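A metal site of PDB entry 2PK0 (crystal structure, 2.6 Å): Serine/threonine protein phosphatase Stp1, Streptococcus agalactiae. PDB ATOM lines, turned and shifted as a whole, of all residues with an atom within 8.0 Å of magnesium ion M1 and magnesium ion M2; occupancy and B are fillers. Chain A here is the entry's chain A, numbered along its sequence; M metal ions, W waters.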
ATOM      1  N   ARG A  18     -26.314  33.566 -18.834  1.00  0.00           N
ATOM      2  CA  ARG A  18     -26.964  32.364 -19.355  1.00  0.00           C
ATOM      3  C   ARG A  18     -28.176  31.923 -18.537  1.00  0.00           C
ATOM      4  O   ARG A  18     -28.274  32.198 -17.340  1.00  0.00           O
ATOM      5  CB  ARG A  18     -25.967  31.227 -19.540  1.00  0.00           C
ATOM      6  CG  ARG A  18     -24.986  31.463 -20.669  1.00  0.00           C
ATOM      7  CD  ARG A  18     -24.739  30.209 -21.464  1.00  0.00           C
ATOM      8  NE  ARG A  18     -23.481  30.285 -22.187  1.00  0.00           N
ATOM      9  CZ  ARG A  18     -22.732  29.225 -22.507  1.00  0.00           C
ATOM     10  NH1 ARG A  18     -23.128  28.015 -22.145  1.00  0.00           N
ATOM     11  NH2 ARG A  18     -21.599  29.395 -23.161  1.00  0.00           N
ATOM     12  N   ASN A  20     -29.378  28.715 -18.546  1.00  0.00           N
ATOM     13  CA  ASN A  20     -29.377  27.283 -18.401  1.00  0.00           C
ATOM     14  C   ASN A  20     -27.994  26.831 -17.947  1.00  0.00           C
ATOM     15  O   ASN A  20     -26.984  27.185 -18.560  1.00  0.00           O
ATOM     16  CB  ASN A  20     -29.769  26.634 -19.730  1.00  0.00           C
ATOM     17  CG  ASN A  20     -30.014  25.162 -19.608  1.00  0.00           C
ATOM     18  OD1 ASN A  20     -29.827  24.410 -20.549  1.00  0.00           O
ATOM     19  ND2 ASN A  20     -30.422  24.743 -18.436  1.00  0.00           N
ATOM     20  N   ASN A  21     -27.962  26.079 -16.863  1.00  0.00           N
ATOM     21  CA  ASN A  21     -26.723  25.538 -16.316  1.00  0.00           C
ATOM     22  C   ASN A  21     -26.512  24.114 -16.801  1.00  0.00           C
ATOM     23  O   ASN A  21     -27.138  23.201 -16.266  1.00  0.00           O
ATOM     24  CB  ASN A  21     -26.779  25.552 -14.787  1.00  0.00           C
ATOM     25  CG  ASN A  21     -25.422  25.268 -14.133  1.00  0.00           C
ATOM     26  OD1 ASN A  21     -24.439  24.956 -14.810  1.00  0.00           O
ATOM     27  ND2 ASN A  21     -25.379  25.383 -12.819  1.00  0.00           N
ATOM     28  N   GLN A  22     -25.625  23.903 -17.764  1.00  0.00           N
ATOM     29  CA  GLN A  22     -25.367  22.553 -18.253  1.00  0.00           C
ATOM     30  C   GLN A  22     -24.116  21.924 -17.612  1.00  0.00           C
ATOM     31  O   GLN A  22     -23.605  20.900 -18.078  1.00  0.00           O
ATOM     32  CB  GLN A  22     -25.257  22.515 -19.783  1.00  0.00           C
ATOM     33  CG  GLN A  22     -26.394  23.214 -20.528  1.00  0.00           C
ATOM     34  CD  GLN A  22     -26.273  23.053 -22.034  1.00  0.00           C
ATOM     35  OE1 GLN A  22     -25.282  23.477 -22.646  1.00  0.00           O
ATOM     36  NE2 GLN A  22     -27.291  22.442 -22.645  1.00  0.00           N
ATOM     37  N   ASP A  23     -23.602  22.551 -16.553  1.00  0.00           N
ATOM     38  CA  ASP A  23     -22.539  21.945 -15.776  1.00  0.00           C
ATOM     39  C   ASP A  23     -23.187  21.040 -14.729  1.00  0.00           C
ATOM     40  O   ASP A  23     -24.301  21.345 -14.276  1.00  0.00           O
ATOM     41  CB  ASP A  23     -21.715  22.999 -15.034  1.00  0.00           C
ATOM     42  CG  ASP A  23     -20.734  23.760 -15.920  1.00  0.00           C
ATOM     43  OD1 ASP A  23     -20.544  23.401 -17.108  1.00  0.00           O
ATOM     44  OD2 ASP A  23     -20.136  24.732 -15.404  1.00  0.00           O
ATOM     45  N   PHE A  24     -22.521  19.949 -14.355  1.00  0.00           N
ATOM     46  CA  PHE A  24     -22.916  19.163 -13.174  1.00  0.00           C
ATOM     47  C   PHE A  24     -21.721  18.802 -12.283  1.00  0.00           C
ATOM     48  O   PHE A  24     -20.648  18.521 -12.784  1.00  0.00           O
ATOM     49  CB  PHE A  24     -23.667  17.878 -13.583  1.00  0.00           C
ATOM     50  CG  PHE A  24     -24.713  17.440 -12.582  1.00  0.00           C
ATOM     51  CD1 PHE A  24     -25.928  18.107 -12.473  1.00  0.00           C
ATOM     52  CD2 PHE A  24     -24.494  16.349 -11.755  1.00  0.00           C
ATOM     53  CE1 PHE A  24     -26.906  17.706 -11.553  1.00  0.00           C
ATOM     54  CE2 PHE A  24     -25.462  15.938 -10.844  1.00  0.00           C
ATOM     55  CZ  PHE A  24     -26.667  16.615 -10.735  1.00  0.00           C
ATOM     56  N   ALA A  40     -18.499  17.909 -14.512  1.00  0.00           N
ATOM     57  CA  ALA A  40     -18.748  17.727 -15.944  1.00  0.00           C
ATOM     58  C   ALA A  40     -19.346  18.933 -16.591  1.00  0.00           C
ATOM     59  O   ALA A  40     -20.303  19.490 -16.086  1.00  0.00           O
ATOM     60  CB  ALA A  40     -19.625  16.531 -16.176  1.00  0.00           C
ATOM     61  N   ASP A  41     -18.797  19.347 -17.720  1.00  0.00           N
ATOM     62  CA  ASP A  41     -19.343  20.474 -18.445  1.00  0.00           C
ATOM     63  C   ASP A  41     -20.024  19.968 -19.734  1.00  0.00           C
ATOM     64  O   ASP A  41     -19.358  19.629 -20.707  1.00  0.00           O
ATOM     65  CB  ASP A  41     -18.235  21.490 -18.731  1.00  0.00           C
ATOM     66  CG  ASP A  41     -18.693  22.694 -19.555  1.00  0.00           C
ATOM     67  OD1 ASP A  41     -19.808  22.737 -20.150  1.00  0.00           O
ATOM     68  OD2 ASP A  41     -17.900  23.647 -19.636  1.00  0.00           O
ATOM     69  N   GLY A  42     -21.355  19.961 -19.743  1.00  0.00           N
ATOM     70  CA  GLY A  42     -22.090  19.524 -20.912  1.00  0.00           C
ATOM     71  C   GLY A  42     -22.262  20.561 -22.015  1.00  0.00           C
ATOM     72  O   GLY A  42     -22.206  21.764 -21.763  1.00  0.00           O
ATOM     73  N   MET A  43     -22.462  20.086 -23.248  1.00  0.00           N
ATOM     74  CA  MET A  43     -22.785  20.935 -24.379  1.00  0.00           C
ATOM     75  C   MET A  43     -23.928  20.332 -25.201  1.00  0.00           C
ATOM     76  O   MET A  43     -24.178  19.120 -25.167  1.00  0.00           O
ATOM     77  CB  MET A  43     -21.553  21.146 -25.248  1.00  0.00           C
ATOM     78  CG  MET A  43     -20.988  19.851 -25.828  1.00  0.00           C
ATOM     79  SD  MET A  43     -19.514  20.084 -26.845  1.00  0.00           S
ATOM     80  CE  MET A  43     -19.569  18.626 -27.904  1.00  0.00           C
ATOM     81  N   GLY A  44     -24.633  21.177 -25.949  1.00  0.00           N
ATOM     82  CA  GLY A  44     -25.727  20.706 -26.805  1.00  0.00           C
ATOM     83  C   GLY A  44     -26.997  21.472 -26.517  1.00  0.00           C
ATOM     84  O   GLY A  44     -27.338  21.673 -25.357  1.00  0.00           O
ATOM     85  N   GLY A  49     -27.078  19.139 -23.139  1.00  0.00           N
ATOM     86  CA  GLY A  49     -25.918  19.432 -22.319  1.00  0.00           C
ATOM     87  C   GLY A  49     -26.188  19.112 -20.868  1.00  0.00           C
ATOM     88  O   GLY A  49     -25.288  18.656 -20.159  1.00  0.00           O
ATOM     89  N   ASN A  50     -27.433  19.339 -20.441  1.00  0.00           N
ATOM     90  CA  ASN A  50     -27.870  19.022 -19.076  1.00  0.00           C
ATOM     91  C   ASN A  50     -27.888  17.532 -18.809  1.00  0.00           C
ATOM     92  O   ASN A  50     -27.373  17.089 -17.791  1.00  0.00           O
ATOM     93  CB  ASN A  50     -29.256  19.592 -18.781  1.00  0.00           C
ATOM     94  CG  ASN A  50     -29.354  21.069 -19.086  1.00  0.00           C
ATOM     95  OD1 ASN A  50     -29.327  21.472 -20.242  1.00  0.00           O
ATOM     96  ND2 ASN A  50     -29.458  21.882 -18.037  1.00  0.00           N
ATOM     97  N   SER A  53     -24.174  15.840 -18.837  1.00  0.00           N
ATOM     98  CA  SER A  53     -23.398  16.183 -17.640  1.00  0.00           C
ATOM     99  C   SER A  53     -23.951  15.505 -16.387  1.00  0.00           C
ATOM    100  O   SER A  53     -23.197  14.873 -15.662  1.00  0.00           O
ATOM    101  CB  SER A  53     -23.309  17.710 -17.451  1.00  0.00           C
ATOM    102  OG  SER A  53     -24.555  18.309 -17.160  1.00  0.00           O
ATOM    103  N   GLY A 103     -22.764  16.144 -25.593  1.00  0.00           N
ATOM    104  CA  GLY A 103     -21.490  15.730 -25.067  1.00  0.00           C
ATOM    105  C   GLY A 103     -21.113  16.466 -23.801  1.00  0.00           C
ATOM    106  O   GLY A 103     -21.719  17.491 -23.469  1.00  0.00           O
ATOM    107  N   THR A 104     -20.116  15.952 -23.095  1.00  0.00           N
ATOM    108  CA  THR A 104     -19.644  16.624 -21.900  1.00  0.00           C
ATOM    109  C   THR A 104     -18.131  16.538 -21.695  1.00  0.00           C
ATOM    110  O   THR A 104     -17.493  15.597 -22.152  1.00  0.00           O
ATOM    111  CB  THR A 104     -20.369  16.111 -20.638  1.00  0.00           C
ATOM    112  OG1 THR A 104     -19.834  16.783 -19.500  1.00  0.00           O
ATOM    113  CG2 THR A 104     -20.177  14.613 -20.460  1.00  0.00           C
ATOM    114  N   THR A 105     -17.542  17.522 -21.025  1.00  0.00           N
ATOM    115  CA  THR A 105     -16.192  17.353 -20.507  1.00  0.00           C
ATOM    116  C   THR A 105     -16.257  16.460 -19.258  1.00  0.00           C
ATOM    117  O   THR A 105     -17.330  16.254 -18.699  1.00  0.00           O
ATOM    118  CB  THR A 105     -15.534  18.682 -20.068  1.00  0.00           C
ATOM    119  OG1 THR A 105     -16.138  19.148 -18.851  1.00  0.00           O
ATOM    120  CG2 THR A 105     -15.635  19.735 -21.132  1.00  0.00           C
ATOM    121  N   ASP A 123     -11.979  20.707 -21.757  1.00  0.00           N
ATOM    122  CA  ASP A 123     -11.320  21.957 -21.389  1.00  0.00           C
ATOM    123  C   ASP A 123     -11.622  22.397 -19.951  1.00  0.00           C
ATOM    124  O   ASP A 123     -11.388  23.544 -19.566  1.00  0.00           O
ATOM    125  CB  ASP A 123     -11.646  23.084 -22.376  1.00  0.00           C
ATOM    126  CG  ASP A 123     -13.138  23.386 -22.461  1.00  0.00           C
ATOM    127  OD1 ASP A 123     -13.956  22.608 -21.910  1.00  0.00           O
ATOM    128  OD2 ASP A 123     -13.495  24.417 -23.094  1.00  0.00           O
ATOM    129  N   SER A 124     -12.148  21.480 -19.153  1.00  0.00           N
ATOM    130  CA  SER A 124     -12.235  21.692 -17.726  1.00  0.00           C
ATOM    131  C   SER A 124     -10.813  21.579 -17.147  1.00  0.00           C
ATOM    132  O   SER A 124      -9.897  21.081 -17.806  1.00  0.00           O
ATOM    133  CB  SER A 124     -13.169  20.684 -17.091  1.00  0.00           C
ATOM    134  OG  SER A 124     -14.519  20.934 -17.425  1.00  0.00           O
ATOM    135  N   SER A 196     -14.732  24.128 -14.230  1.00  0.00           N
ATOM    136  CA  SER A 196     -15.153  24.150 -15.633  1.00  0.00           C
ATOM    137  C   SER A 196     -14.594  25.444 -16.165  1.00  0.00           C
ATOM    138  O   SER A 196     -14.131  26.278 -15.382  1.00  0.00           O
ATOM    139  CB  SER A 196     -16.667  24.153 -15.742  1.00  0.00           C
ATOM    140  OG  SER A 196     -17.217  25.277 -15.093  1.00  0.00           O
ATOM    141  N   ASP A 197     -14.656  25.643 -17.493  1.00  0.00           N
ATOM    142  CA  ASP A 197     -13.969  26.770 -18.100  1.00  0.00           C
ATOM    143  C   ASP A 197     -14.505  28.134 -17.671  1.00  0.00           C
ATOM    144  O   ASP A 197     -13.801  29.128 -17.765  1.00  0.00           O
ATOM    145  CB  ASP A 197     -13.880  26.652 -19.632  1.00  0.00           C
ATOM    146  CG  ASP A 197     -15.238  26.433 -20.315  1.00  0.00           C
ATOM    147  OD1 ASP A 197     -16.247  26.235 -19.604  1.00  0.00           O
ATOM    148  OD2 ASP A 197     -15.326  26.441 -21.566  1.00  0.00           O
ATOM    149  N   GLY A 198     -15.728  28.163 -17.153  1.00  0.00           N
ATOM    150  CA  GLY A 198     -16.368  29.401 -16.746  1.00  0.00           C
ATOM    151  C   GLY A 198     -15.663  30.122 -15.601  1.00  0.00           C
ATOM    152  O   GLY A 198     -15.827  31.322 -15.435  1.00  0.00           O
ATOM    153  N   LEU A 199     -14.892  29.389 -14.817  1.00  0.00           N
ATOM    154  CA  LEU A 199     -14.072  30.021 -13.799  1.00  0.00           C
ATOM    155  C   LEU A 199     -12.851  30.626 -14.458  1.00  0.00           C
ATOM    156  O   LEU A 199     -12.653  31.837 -14.425  1.00  0.00           O
ATOM    157  CB  LEU A 199     -13.645  29.028 -12.710  1.00  0.00           C
ATOM    158  CG  LEU A 199     -12.947  29.755 -11.539  1.00  0.00           C
ATOM    159  CD1 LEU A 199     -13.970  30.536 -10.738  1.00  0.00           C
ATOM    160  CD2 LEU A 199     -12.180  28.788 -10.630  1.00  0.00           C
ATOM    161  N   ASN A 201     -11.937  31.119 -17.595  1.00  0.00           N
ATOM    162  CA  ASN A 201     -12.060  32.095 -18.676  1.00  0.00           C
ATOM    163  C   ASN A 201     -12.263  33.498 -18.132  1.00  0.00           C
ATOM    164  O   ASN A 201     -11.907  34.468 -18.772  1.00  0.00           O
ATOM    165  CB  ASN A 201     -13.193  31.740 -19.639  1.00  0.00           C
ATOM    166  CG  ASN A 201     -12.915  30.476 -20.453  1.00  0.00           C
ATOM    167  OD1 ASN A 201     -11.772  29.993 -20.559  1.00  0.00           O
ATOM    168  ND2 ASN A 201     -13.969  29.932 -21.038  1.00  0.00           N
ATOM    169  N   LEU A 235     -19.934  34.874 -18.451  1.00  0.00           N
ATOM    170  CA  LEU A 235     -20.409  34.473 -19.774  1.00  0.00           C
ATOM    171  C   LEU A 235     -20.718  32.998 -19.941  1.00  0.00           C
ATOM    172  O   LEU A 235     -21.248  32.598 -20.962  1.00  0.00           O
ATOM    173  CB  LEU A 235     -19.415  34.866 -20.854  1.00  0.00           C
ATOM    174  CG  LEU A 235     -19.003  36.330 -20.956  1.00  0.00           C
ATOM    175  CD1 LEU A 235     -18.126  36.505 -22.153  1.00  0.00           C
ATOM    176  CD2 LEU A 235     -20.188  37.249 -21.044  1.00  0.00           C
ATOM    177  N   ASP A 236     -20.399  32.191 -18.950  1.00  0.00           N
ATOM    178  CA  ASP A 236     -20.599  30.764 -19.053  1.00  0.00           C
ATOM    179  C   ASP A 236     -20.922  30.258 -17.663  1.00  0.00           C
ATOM    180  O   ASP A 236     -20.731  30.986 -16.697  1.00  0.00           O
ATOM    181  CB  ASP A 236     -19.350  30.095 -19.628  1.00  0.00           C
ATOM    182  CG  ASP A 236     -19.539  28.617 -19.964  1.00  0.00           C
ATOM    183  OD1 ASP A 236     -20.662  28.080 -19.868  1.00  0.00           O
ATOM    184  OD2 ASP A 236     -18.549  27.968 -20.308  1.00  0.00           O
ATOM    185  N   ASN A 237     -21.458  29.032 -17.585  1.00  0.00           N
ATOM    186  CA  ASN A 237     -21.665  28.353 -16.316  1.00  0.00           C
ATOM    187  C   ASN A 237     -20.352  28.183 -15.589  1.00  0.00           C
ATOM    188  O   ASN A 237     -19.353  27.820 -16.196  1.00  0.00           O
ATOM    189  CB  ASN A 237     -22.301  26.982 -16.534  1.00  0.00           C
ATOM    190  CG  ASN A 237     -23.557  27.030 -17.374  1.00  0.00           C
ATOM    191  OD1 ASN A 237     -23.803  26.137 -18.187  1.00  0.00           O
ATOM    192  ND2 ASN A 237     -24.382  28.052 -17.157  1.00  0.00           N
ATOM    193  N   ILE A 238     -20.341  28.482 -14.291  1.00  0.00           N
ATOM    194  CA  ILE A 238     -19.131  28.351 -13.467  1.00  0.00           C
ATOM    195  C   ILE A 238     -19.359  27.243 -12.476  1.00  0.00           C
ATOM    196  O   ILE A 238     -20.423  27.196 -11.856  1.00  0.00           O
ATOM    197  CB  ILE A 238     -18.905  29.607 -12.658  1.00  0.00           C
ATOM    198  CG1 ILE A 238     -19.283  30.840 -13.489  1.00  0.00           C
ATOM    199  CG2 ILE A 238     -17.497  29.655 -12.198  1.00  0.00           C
ATOM    200  CD1 ILE A 238     -19.709  32.022 -12.645  1.00  0.00           C
ATOM    201  N   THR A 239     -18.387  26.355 -12.306  1.00  0.00           N
ATOM    202  CA  THR A 239     -18.563  25.180 -11.451  1.00  0.00           C
ATOM    203  C   THR A 239     -17.224  24.798 -10.869  1.00  0.00           C
ATOM    204  O   THR A 239     -16.268  24.617 -11.616  1.00  0.00           O
ATOM    205  CB  THR A 239     -19.152  24.011 -12.250  1.00  0.00           C
ATOM    206  OG1 THR A 239     -20.518  24.318 -12.587  1.00  0.00           O
ATOM    207  CG2 THR A 239     -19.141  22.739 -11.445  1.00  0.00           C
HETATM  208 MG    MG M   1     -18.223  25.855 -20.055  1.00  0.00          MG
HETATM  209 MG    MG M   2     -21.294  23.483 -21.158  1.00  0.00          MG
HETATM  210  O   HOH W   1     -17.797  25.644 -22.163  1.00  0.00           O
HETATM  211  O   HOH W   2     -20.100  23.802 -23.061  1.00  0.00           O
HETATM  212  O   HOH W   3     -19.144  25.539 -18.134  1.00  0.00           O
HETATM  213  O   HOH W   4     -20.195  25.359 -20.877  1.00  0.00           O
HETATM  214  O   HOH W   5     -22.481  24.448 -22.179  1.00  0.00           O
HETATM  215  O   HOH W   6     -21.957  24.089 -19.304  1.00  0.00           O
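OD1 of Asp 197 binds magnesium ion M1 (2.1 Å). OD2 of Asp 236 binds magnesium ion M1, 2.2 Å away. Water W3 is bound to magnesium ion M1 (2.2 Å). Water W1 is bound to magnesium ion M1, at 2.2 Å. Water W4 binds magnesium ion M1. Magnesium ion M1 is bound by OD2 of Asp 41, at 2.3 Å.
Three residues have an atom within 4 Å of magnesium ion M1: Asp 41, Asp 197 and Asp 236. Along chain A the residues within 4 Å of magnesium ion M1 span positions 41 to 236. The nearest printed residue that does not touch magnesium ion M1 is Gly 198 (4.5 Å).
OD1 of Asp 236 lies within salt-bridge range of NH1 of Arg 18, 3.4 Å away. The backbone NH (N) of Gly 42 lies within hydrogen-bond range of the backbone carbonyl oxygen (O) of Gln 22, 3.0 Å away. ND2 of Asn 201 lies close to O of Asp 197. O of Asp 41 is in hydrogen-bond range of OG1 of Thr 104 (3.1 Å). N of Thr 105 sits at hydrogen-bond distance from O of Asp 41, 2.8 Å away.
Magnesium ion M2 is bound by water W5 (1.8 Å), the side-chain carboxylate of Asp 41 (1.9 Å), the backbone carbonyl oxygen of Gly 42 (2.0 Å), water W6 (2.1 Å), water W4 (2.2 Å) and water W2 (2.3 Å).
Within 4 Å of magnesium ion M2: Asp 41 and Gly 42. The nearest printed residue that does not touch magnesium ion M2 is Asp 23 (4.1 Å).
Water W6 bridges the side-chain carboxylate (OD1) of Asp 23 (2.7 Å) and the side-chain amide oxygen (OD1) of Asn 237 (3.0 Å).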
